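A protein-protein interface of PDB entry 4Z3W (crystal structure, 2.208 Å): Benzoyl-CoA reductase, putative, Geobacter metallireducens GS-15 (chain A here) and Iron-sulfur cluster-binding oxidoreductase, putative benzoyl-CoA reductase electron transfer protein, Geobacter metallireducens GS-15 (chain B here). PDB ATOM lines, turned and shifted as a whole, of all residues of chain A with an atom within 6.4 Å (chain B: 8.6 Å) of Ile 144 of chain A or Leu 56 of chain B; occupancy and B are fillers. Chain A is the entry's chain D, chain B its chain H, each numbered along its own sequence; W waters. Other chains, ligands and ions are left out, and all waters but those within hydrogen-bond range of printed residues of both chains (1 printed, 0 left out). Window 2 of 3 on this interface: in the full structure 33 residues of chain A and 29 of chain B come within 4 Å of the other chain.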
ATOM      1  N   LYS A 141       2.747  23.358  32.776  1.00  0.00           N
ATOM      2  CA  LYS A 141       2.844  23.488  31.317  1.00  0.00           C
ATOM      3  C   LYS A 141       2.013  22.420  30.618  1.00  0.00           C
ATOM      4  O   LYS A 141       1.954  21.277  31.075  1.00  0.00           O
ATOM      5  CB  LYS A 141       4.297  23.392  30.840  1.00  0.00           C
ATOM      6  CG  LYS A 141       5.246  24.402  31.479  1.00  0.00           C
ATOM      7  CD  LYS A 141       5.574  25.538  30.534  1.00  0.00           C
ATOM      8  CE  LYS A 141       6.369  26.617  31.254  1.00  0.00           C
ATOM      9  NZ  LYS A 141       7.037  27.533  30.308  1.00  0.00           N
ATOM     10  N   GLY A 142       1.382  22.808  29.508  1.00  0.00           N
ATOM     11  CA  GLY A 142       0.618  21.902  28.673  1.00  0.00           C
ATOM     12  C   GLY A 142       1.385  20.649  28.290  1.00  0.00           C
ATOM     13  O   GLY A 142       2.619  20.629  28.298  1.00  0.00           O
ATOM     14  N   ALA A 143       0.645  19.604  27.941  1.00  0.00           N
ATOM     15  CA  ALA A 143       1.238  18.299  27.690  1.00  0.00           C
ATOM     16  C   ALA A 143       2.110  18.297  26.436  1.00  0.00           C
ATOM     17  O   ALA A 143       3.172  17.675  26.418  1.00  0.00           O
ATOM     18  CB  ALA A 143       0.144  17.235  27.577  1.00  0.00           C
ATOM     19  N   ILE A 144       1.667  18.983  25.388  1.00  0.00           N
ATOM     20  CA  ILE A 144       2.458  19.060  24.166  1.00  0.00           C
ATOM     21  C   ILE A 144       3.608  20.056  24.361  1.00  0.00           C
ATOM     22  O   ILE A 144       4.771  19.763  24.054  1.00  0.00           O
ATOM     23  CB  ILE A 144       1.598  19.469  22.949  1.00  0.00           C
ATOM     24  CG1 ILE A 144       0.436  18.501  22.757  1.00  0.00           C
ATOM     25  CG2 ILE A 144       2.430  19.442  21.683  1.00  0.00           C
ATOM     26  CD1 ILE A 144       0.888  17.134  22.264  1.00  0.00           C
ATOM     27  N   GLU A 145       3.270  21.227  24.889  1.00  0.00           N
ATOM     28  CA  GLU A 145       4.251  22.247  25.250  1.00  0.00           C
ATOM     29  C   GLU A 145       5.430  21.652  26.036  1.00  0.00           C
ATOM     30  O   GLU A 145       6.592  21.875  25.693  1.00  0.00           O
ATOM     31  CB  GLU A 145       3.556  23.348  26.060  1.00  0.00           C
ATOM     32  CG  GLU A 145       4.402  24.546  26.414  1.00  0.00           C
ATOM     33  CD  GLU A 145       3.677  25.487  27.368  1.00  0.00           C
ATOM     34  OE1 GLU A 145       2.562  25.134  27.822  1.00  0.00           O
ATOM     35  OE2 GLU A 145       4.222  26.572  27.668  1.00  0.00           O
ATOM     36  N   THR A 146       5.110  20.883  27.080  1.00  0.00           N
ATOM     37  CA  THR A 146       6.099  20.201  27.916  1.00  0.00           C
ATOM     38  C   THR A 146       7.036  19.322  27.095  1.00  0.00           C
ATOM     39  O   THR A 146       8.241  19.259  27.356  1.00  0.00           O
ATOM     40  CB  THR A 146       5.409  19.313  29.002  1.00  0.00           C
ATOM     41  OG1 THR A 146       4.687  20.135  29.933  1.00  0.00           O
ATOM     42  CG2 THR A 146       6.428  18.475  29.759  1.00  0.00           C
ATOM     43  N   ALA A 147       6.486  18.642  26.099  1.00  0.00           N
ATOM     44  CA  ALA A 147       7.283  17.724  25.301  1.00  0.00           C
ATOM     45  C   ALA A 147       8.356  18.468  24.511  1.00  0.00           C
ATOM     46  O   ALA A 147       9.470  17.972  24.364  1.00  0.00           O
ATOM     47  CB  ALA A 147       6.397  16.930  24.368  1.00  0.00           C
ATOM     48  N   GLU A 148       8.026  19.654  24.009  1.00  0.00           N
ATOM     49  CA  GLU A 148       8.964  20.404  23.169  1.00  0.00           C
ATOM     50  C   GLU A 148      10.105  20.994  24.005  1.00  0.00           C
ATOM     51  O   GLU A 148      11.272  20.864  23.655  1.00  0.00           O
ATOM     52  CB  GLU A 148       8.234  21.503  22.398  1.00  0.00           C
ATOM     53  CG  GLU A 148       7.172  20.971  21.448  1.00  0.00           C
ATOM     54  CD  GLU A 148       7.744  20.027  20.398  1.00  0.00           C
ATOM     55  OE1 GLU A 148       8.773  20.387  19.777  1.00  0.00           O
ATOM     56  OE2 GLU A 148       7.162  18.930  20.195  1.00  0.00           O
ATOM     57  N   ILE A 149       9.753  21.636  25.114  1.00  0.00           N
ATOM     58  CA  ILE A 149      10.729  22.106  26.090  1.00  0.00           C
ATOM     59  C   ILE A 149      11.700  21.006  26.532  1.00  0.00           C
ATOM     60  O   ILE A 149      12.903  21.236  26.614  1.00  0.00           O
ATOM     61  CB  ILE A 149      10.025  22.675  27.331  1.00  0.00           C
ATOM     62  CG1 ILE A 149       9.192  23.898  26.942  1.00  0.00           C
ATOM     63  CG2 ILE A 149      11.034  23.015  28.417  1.00  0.00           C
ATOM     64  CD1 ILE A 149       8.107  24.239  27.946  1.00  0.00           C
ATOM     65  N   LYS A 151      12.535  18.235  24.910  1.00  0.00           N
ATOM     66  CA  LYS A 151      13.384  17.807  23.799  1.00  0.00           C
ATOM     67  C   LYS A 151      14.523  18.795  23.522  1.00  0.00           C
ATOM     68  O   LYS A 151      15.649  18.378  23.236  1.00  0.00           O
ATOM     69  CB  LYS A 151      12.544  17.571  22.541  1.00  0.00           C
ATOM     70  CG  LYS A 151      11.634  16.336  22.680  1.00  0.00           C
ATOM     71  CD  LYS A 151      10.918  15.984  21.396  1.00  0.00           C
ATOM     72  CE  LYS A 151       9.902  17.034  21.027  1.00  0.00           C
ATOM     73  NZ  LYS A 151       9.172  16.657  19.780  1.00  0.00           N
ATOM     74  N   ALA A 163       3.261  12.892  28.182  1.00  0.00           N
ATOM     75  CA  ALA A 163       3.169  13.844  29.284  1.00  0.00           C
ATOM     76  C   ALA A 163       1.742  14.107  29.753  1.00  0.00           C
ATOM     77  O   ALA A 163       0.766  13.857  29.041  1.00  0.00           O
ATOM     78  CB  ALA A 163       3.820  15.159  28.894  1.00  0.00           C
ATOM     79  N   GLU A 178      -0.735  12.757  27.066  1.00  0.00           N
ATOM     80  CA  GLU A 178      -0.684  13.143  25.653  1.00  0.00           C
ATOM     81  C   GLU A 178       0.700  12.980  25.035  1.00  0.00           C
ATOM     82  O   GLU A 178       1.718  13.271  25.670  1.00  0.00           O
ATOM     83  CB  GLU A 178      -1.150  14.596  25.477  1.00  0.00           C
ATOM     84  CG  GLU A 178      -2.528  14.903  26.091  1.00  0.00           C
ATOM     85  CD  GLU A 178      -3.690  14.304  25.289  1.00  0.00           C
ATOM     86  OE1 GLU A 178      -3.529  14.063  24.069  1.00  0.00           O
ATOM     87  OE2 GLU A 178      -4.765  14.069  25.882  1.00  0.00           O
ATOM     88  N   GLN A 179       0.722  12.520  23.789  1.00  0.00           N
ATOM     89  CA  GLN A 179       1.960  12.351  23.040  1.00  0.00           C
ATOM     90  C   GLN A 179       1.746  12.633  21.560  1.00  0.00           C
ATOM     91  O   GLN A 179       1.205  11.788  20.843  1.00  0.00           O
ATOM     92  CB  GLN A 179       2.509  10.936  23.214  1.00  0.00           C
ATOM     93  CG  GLN A 179       3.749  10.664  22.357  1.00  0.00           C
ATOM     94  CD  GLN A 179       3.506   9.605  21.290  1.00  0.00           C
ATOM     95  OE1 GLN A 179       2.891   8.562  21.554  1.00  0.00           O
ATOM     96  NE2 GLN A 179       3.978   9.872  20.075  1.00  0.00           N
ATOM     97  N   GLY A 180       2.162  13.809  21.098  1.00  0.00           N
ATOM     98  CA  GLY A 180       1.935  14.185  19.710  1.00  0.00           C
ATOM     99  C   GLY A 180       0.454  14.098  19.363  1.00  0.00           C
ATOM    100  O   GLY A 180      -0.371  14.821  19.924  1.00  0.00           O
ATOM    101  N   ARG A 181       0.098  13.195  18.458  1.00  0.00           N
ATOM    102  CA  ARG A 181      -1.284  13.147  17.976  1.00  0.00           C
ATOM    103  C   ARG A 181      -2.032  11.933  18.586  1.00  0.00           C
ATOM    104  O   ARG A 181      -3.003  11.407  18.040  1.00  0.00           O
ATOM    105  CB  ARG A 181      -1.291  13.162  16.435  1.00  0.00           C
ATOM    106  CG  ARG A 181      -1.050  11.852  15.712  1.00  0.00           C
ATOM    107  CD  ARG A 181      -2.418  11.204  15.456  1.00  0.00           C
ATOM    108  NE  ARG A 181      -2.469  10.332  14.300  1.00  0.00           N
ATOM    109  CZ  ARG A 181      -3.252   9.268  14.214  1.00  0.00           C
ATOM    110  NH1 ARG A 181      -4.040   8.917  15.227  1.00  0.00           N
ATOM    111  NH2 ARG A 181      -3.229   8.543  13.113  1.00  0.00           N
ATOM    112  N   SER A 182      -1.582  11.558  19.775  1.00  0.00           N
ATOM    113  CA  SER A 182      -1.982  10.348  20.445  1.00  0.00           C
ATOM    114  C   SER A 182      -2.301  10.619  21.904  1.00  0.00           C
ATOM    115  O   SER A 182      -1.712  11.499  22.524  1.00  0.00           O
ATOM    116  CB  SER A 182      -0.874   9.303  20.332  1.00  0.00           C
ATOM    117  OG  SER A 182      -0.633   9.013  18.967  1.00  0.00           O
ATOM    118  N   THR A 309      -3.276  17.596  12.109  1.00  0.00           N
ATOM    119  CA  THR A 309      -2.831  18.775  12.830  1.00  0.00           C
ATOM    120  C   THR A 309      -3.918  19.825  12.648  1.00  0.00           C
ATOM    121  O   THR A 309      -4.454  19.974  11.546  1.00  0.00           O
ATOM    122  CB  THR A 309      -1.478  19.331  12.295  1.00  0.00           C
ATOM    123  OG1 THR A 309      -1.468  19.264  10.864  1.00  0.00           O
ATOM    124  CG2 THR A 309      -0.297  18.545  12.830  1.00  0.00           C
ATOM    125  N   THR A 317      -0.823  25.123  17.404  1.00  0.00           N
ATOM    126  CA  THR A 317      -1.267  23.935  16.710  1.00  0.00           C
ATOM    127  C   THR A 317      -1.446  22.802  17.710  1.00  0.00           C
ATOM    128  O   THR A 317      -0.753  22.756  18.720  1.00  0.00           O
ATOM    129  CB  THR A 317      -0.270  23.533  15.617  1.00  0.00           C
ATOM    130  OG1 THR A 317      -0.276  24.543  14.606  1.00  0.00           O
ATOM    131  CG2 THR A 317      -0.649  22.197  14.986  1.00  0.00           C
ATOM    132  N   TYR A 318      -2.406  21.919  17.443  1.00  0.00           N
ATOM    133  CA  TYR A 318      -2.538  20.668  18.179  1.00  0.00           C
ATOM    134  C   TYR A 318      -3.001  19.598  17.211  1.00  0.00           C
ATOM    135  O   TYR A 318      -3.273  19.890  16.051  1.00  0.00           O
ATOM    136  CB  TYR A 318      -3.509  20.792  19.362  1.00  0.00           C
ATOM    137  CG  TYR A 318      -4.991  20.914  19.016  1.00  0.00           C
ATOM    138  CD1 TYR A 318      -5.507  22.068  18.414  1.00  0.00           C
ATOM    139  CD2 TYR A 318      -5.879  19.884  19.323  1.00  0.00           C
ATOM    140  CE1 TYR A 318      -6.864  22.181  18.115  1.00  0.00           C
ATOM    141  CE2 TYR A 318      -7.233  19.990  19.033  1.00  0.00           C
ATOM    142  CZ  TYR A 318      -7.718  21.139  18.436  1.00  0.00           C
ATOM    143  OH  TYR A 318      -9.064  21.233  18.163  1.00  0.00           O
ATOM    144  N   MET A 319      -3.081  18.361  17.685  1.00  0.00           N
ATOM    145  CA  MET A 319      -3.474  17.251  16.831  1.00  0.00           C
ATOM    146  C   MET A 319      -4.763  16.594  17.328  1.00  0.00           C
ATOM    147  O   MET A 319      -5.027  16.573  18.527  1.00  0.00           O
ATOM    148  CB  MET A 319      -2.345  16.226  16.747  1.00  0.00           C
ATOM    149  CG  MET A 319      -1.224  16.639  15.791  1.00  0.00           C
ATOM    150  SD  MET A 319       0.397  16.677  16.583  1.00  0.00           S
ATOM    151  CE  MET A 319       0.101  17.950  17.807  1.00  0.00           C
ATOM    152  N   THR A 347      -6.909  19.666  25.258  1.00  0.00           N
ATOM    153  CA  THR A 347      -5.819  18.743  24.932  1.00  0.00           C
ATOM    154  C   THR A 347      -4.520  19.133  25.650  1.00  0.00           C
ATOM    155  O   THR A 347      -3.759  18.266  26.098  1.00  0.00           O
ATOM    156  CB  THR A 347      -5.545  18.665  23.421  1.00  0.00           C
ATOM    157  OG1 THR A 347      -6.694  18.133  22.751  1.00  0.00           O
ATOM    158  CG2 THR A 347      -4.345  17.754  23.152  1.00  0.00           C
ATOM    159  N   GLU A 348      -4.272  20.433  25.783  1.00  0.00           N
ATOM    160  CA  GLU A 348      -3.046  20.883  26.439  1.00  0.00           C
ATOM    161  C   GLU A 348      -3.114  20.591  27.937  1.00  0.00           C
ATOM    162  O   GLU A 348      -2.207  19.963  28.503  1.00  0.00           O
ATOM    163  CB  GLU A 348      -2.797  22.375  26.179  1.00  0.00           C
ATOM    164  CG  GLU A 348      -1.880  22.664  24.980  1.00  0.00           C
ATOM    165  CD  GLU A 348      -0.448  22.165  25.188  1.00  0.00           C
ATOM    166  OE1 GLU A 348       0.426  22.972  25.590  1.00  0.00           O
ATOM    167  OE2 GLU A 348      -0.193  20.964  24.946  1.00  0.00           O
ATOM    168  N   ARG B  53      10.656  15.188  10.559  1.00  0.00           N
ATOM    169  CA  ARG B  53       9.252  15.110  10.926  1.00  0.00           C
ATOM    170  C   ARG B  53       8.960  16.043  12.081  1.00  0.00           C
ATOM    171  O   ARG B  53       9.349  15.771  13.213  1.00  0.00           O
ATOM    172  CB  ARG B  53       8.888  13.670  11.307  1.00  0.00           C
ATOM    173  CG  ARG B  53       7.396  13.431  11.482  1.00  0.00           C
ATOM    174  CD  ARG B  53       7.062  12.136  12.241  1.00  0.00           C
ATOM    175  NE  ARG B  53       5.625  12.095  12.486  1.00  0.00           N
ATOM    176  CZ  ARG B  53       5.050  12.440  13.633  1.00  0.00           C
ATOM    177  NH1 ARG B  53       5.788  12.799  14.671  1.00  0.00           N
ATOM    178  NH2 ARG B  53       3.736  12.394  13.752  1.00  0.00           N
ATOM    179  N   ASP B  54       8.297  17.156  11.816  1.00  0.00           N
ATOM    180  CA  ASP B  54       7.872  17.997  12.923  1.00  0.00           C
ATOM    181  C   ASP B  54       6.481  18.517  12.659  1.00  0.00           C
ATOM    182  O   ASP B  54       6.310  19.541  11.995  1.00  0.00           O
ATOM    183  CB  ASP B  54       8.833  19.163  13.162  1.00  0.00           C
ATOM    184  CG  ASP B  54       8.496  19.945  14.435  1.00  0.00           C
ATOM    185  OD1 ASP B  54       7.404  19.733  15.017  1.00  0.00           O
ATOM    186  OD2 ASP B  54       9.318  20.782  14.856  1.00  0.00           O
ATOM    187  N   PRO B  55       5.486  17.824  13.225  1.00  0.00           N
ATOM    188  CA  PRO B  55       4.059  18.111  13.054  1.00  0.00           C
ATOM    189  C   PRO B  55       3.738  19.550  13.403  1.00  0.00           C
ATOM    190  O   PRO B  55       2.928  20.178  12.727  1.00  0.00           O
ATOM    191  CB  PRO B  55       3.378  17.145  14.040  1.00  0.00           C
ATOM    192  CG  PRO B  55       4.408  16.052  14.300  1.00  0.00           C
ATOM    193  CD  PRO B  55       5.739  16.744  14.198  1.00  0.00           C
ATOM    194  N   LEU B  56       4.391  20.071  14.438  1.00  0.00           N
ATOM    195  CA  LEU B  56       4.135  21.437  14.897  1.00  0.00           C
ATOM    196  C   LEU B  56       4.721  22.521  13.964  1.00  0.00           C
ATOM    197  O   LEU B  56       4.393  23.698  14.099  1.00  0.00           O
ATOM    198  CB  LEU B  56       4.667  21.604  16.323  1.00  0.00           C
ATOM    199  CG  LEU B  56       4.048  20.589  17.297  1.00  0.00           C
ATOM    200  CD1 LEU B  56       4.636  20.683  18.703  1.00  0.00           C
ATOM    201  CD2 LEU B  56       2.534  20.763  17.338  1.00  0.00           C
ATOM    202  N   ARG B  57       5.570  22.123  13.016  1.00  0.00           N
ATOM    203  CA  ARG B  57       6.034  23.041  11.969  1.00  0.00           C
ATOM    204  C   ARG B  57       5.475  22.642  10.602  1.00  0.00           C
ATOM    205  O   ARG B  57       5.804  23.254   9.584  1.00  0.00           O
ATOM    206  CB  ARG B  57       7.566  23.082  11.901  1.00  0.00           C
ATOM    207  CG  ARG B  57       8.251  23.967  12.928  1.00  0.00           C
ATOM    208  CD  ARG B  57       9.778  23.888  12.778  1.00  0.00           C
ATOM    209  NE  ARG B  57      10.309  22.639  13.310  1.00  0.00           N
ATOM    210  CZ  ARG B  57      11.524  22.166  13.047  1.00  0.00           C
ATOM    211  NH1 ARG B  57      12.342  22.832  12.233  1.00  0.00           N
ATOM    212  NH2 ARG B  57      11.918  21.015  13.597  1.00  0.00           N
ATOM    213  N   ASP B  58       4.622  21.622  10.590  1.00  0.00           N
ATOM    214  CA  ASP B  58       4.125  21.021   9.350  1.00  0.00           C
ATOM    215  C   ASP B  58       5.292  20.664   8.436  1.00  0.00           C
ATOM    216  O   ASP B  58       5.271  20.936   7.229  1.00  0.00           O
ATOM    217  CB  ASP B  58       3.143  21.953   8.631  1.00  0.00           C
ATOM    218  CG  ASP B  58       2.495  21.294   7.414  1.00  0.00           C
ATOM    219  OD1 ASP B  58       1.934  20.186   7.545  1.00  0.00           O
ATOM    220  OD2 ASP B  58       2.592  21.862   6.312  1.00  0.00           O
ATOM    221  N   ILE B  59       6.324  20.053   9.007  1.00  0.00           N
ATOM    222  CA  ILE B  59       7.455  19.641   8.192  1.00  0.00           C
ATOM    223  C   ILE B  59       7.515  18.133   8.126  1.00  0.00           C
ATOM    224  O   ILE B  59       7.566  17.461   9.147  1.00  0.00           O
ATOM    225  CB  ILE B  59       8.782  20.205   8.736  1.00  0.00           C
ATOM    226  CG1 ILE B  59       8.768  21.727   8.629  1.00  0.00           C
ATOM    227  CG2 ILE B  59       9.949  19.644   7.963  1.00  0.00           C
ATOM    228  CD1 ILE B  59       9.901  22.405   9.373  1.00  0.00           C
ATOM    229  N   TYR B  60       7.463  17.607   6.910  1.00  0.00           N
ATOM    230  CA  TYR B  60       7.601  16.178   6.688  1.00  0.00           C
ATOM    231  C   TYR B  60       8.392  16.007   5.407  1.00  0.00           C
ATOM    232  O   TYR B  60       7.840  16.110   4.311  1.00  0.00           O
ATOM    233  CB  TYR B  60       6.242  15.484   6.591  1.00  0.00           C
ATOM    234  CG  TYR B  60       5.272  15.882   7.675  1.00  0.00           C
ATOM    235  CD1 TYR B  60       4.638  17.113   7.637  1.00  0.00           C
ATOM    236  CD2 TYR B  60       4.973  15.014   8.730  1.00  0.00           C
ATOM    237  CE1 TYR B  60       3.752  17.494   8.626  1.00  0.00           C
ATOM    238  CE2 TYR B  60       4.066  15.379   9.731  1.00  0.00           C
ATOM    239  CZ  TYR B  60       3.464  16.623   9.666  1.00  0.00           C
ATOM    240  OH  TYR B  60       2.578  17.019  10.640  1.00  0.00           O
ATOM    241  N   LYS B  84       8.402  28.452   6.816  1.00  0.00           N
ATOM    242  CA  LYS B  84       8.860  27.334   7.630  1.00  0.00           C
ATOM    243  C   LYS B  84      10.339  27.481   7.984  1.00  0.00           C
ATOM    244  O   LYS B  84      11.177  27.659   7.095  1.00  0.00           O
ATOM    245  CB  LYS B  84       8.623  26.009   6.900  1.00  0.00           C
ATOM    246  CG  LYS B  84       7.161  25.731   6.582  1.00  0.00           C
ATOM    247  CD  LYS B  84       6.967  24.311   6.046  1.00  0.00           C
ATOM    248  CE  LYS B  84       5.517  23.874   6.183  1.00  0.00           C
ATOM    249  NZ  LYS B  84       5.223  22.705   5.316  1.00  0.00           N
HETATM  250  O   HOH W   1       1.182  19.476  10.369  1.00  0.00           O
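N of Ile 144 of chain A is in hydrogen-bond range of OE2 of Glu 348 of chain A.
OE2 of Glu 148 of chain A lies within salt-bridge range of NZ of Lys 151 of chain A (3.1 Å).
The backbone NH of Leu 56 of chain B sits at hydrogen-bond distance from the side-chain carboxylate of Asp 54 of chain B (3.1 Å).
Among the printed residues, pairs that only touch across the chains: Ile 144 of chain A with Leu 56 of chain B, Glu 148 of chain A with Leu 56 of chain B, Thr 309 of chain A with Pro 55 of chain B, Thr 309 of chain A with Tyr 60 of chain B, Met 319 of chain A with Pro 55 of chain B and Met 319 of chain A with Leu 56 of chain B.
Ile 144 of chain A touches just one residue of chain B: Leu 56 (3.9 Å).
Leu 56 of chain B touches just these residues of chain A: Ile 144 (3.9 Å), Glu 148 (3.4 Å) and Met 319 (3.7 Å).
Ala 143 of chain A touches none of the printed residues of chain B.
No residue of chain B comes within 4 Å of Gly 180 of chain A.
Printed residues of chain B within 4 Å of Glu 148 of chain A: Leu 56 (3.4 Å).
Printed residues of chain B within 4 Å of Thr 309 of chain A: Pro 55 (3.6 Å) and Tyr 60 (3.9 Å).
Printed residues of chain B within 4 Å of Met 319 of chain A: Pro 55 and Leu 56.
Of the printed residues of chain A, Pro 55 of chain B touches Thr 309 (3.6 Å) and Met 319 (3.9 Å).
Printed residues of chain A within 4 Å of Tyr 60 of chain B: Thr 309 (3.9 Å).
Glu 348 of chain A touches none of the printed residues of chain B.
Arg 53 of chain B touches none of the printed residues of chain A.
Of the 9 printed residues of chain B, 3 touch a printed residue of chain A.
Hydrophobic or aromatic side chains of chain B that line the printed part of chain A: Pro 55, Leu 56 and Tyr 60.
Printed residues of chain A that touch a printed residue of chain B: Ile 144, Glu 148, Thr 309 and Met 319.
Hydrophobic or aromatic side chains of chain A within 4 Å of the printed part of chain B: Ile 144 and Met 319.
Among the printed residues, 6 pairs touch across the chains.
Water W1 lies within hydrogen-bond range of the side-chain hydroxyl (OG1) of Thr 309 of chain A (2.7 Å), the side-chain hydroxyl (OH) of Tyr 60 of chain B (2.8 Å), the side-chain carboxylate (OD1) of Asp 58 of chain B (3.0 Å) and the backbone carbonyl oxygen (O) of Pro 55 of chain B (3.0 Å).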
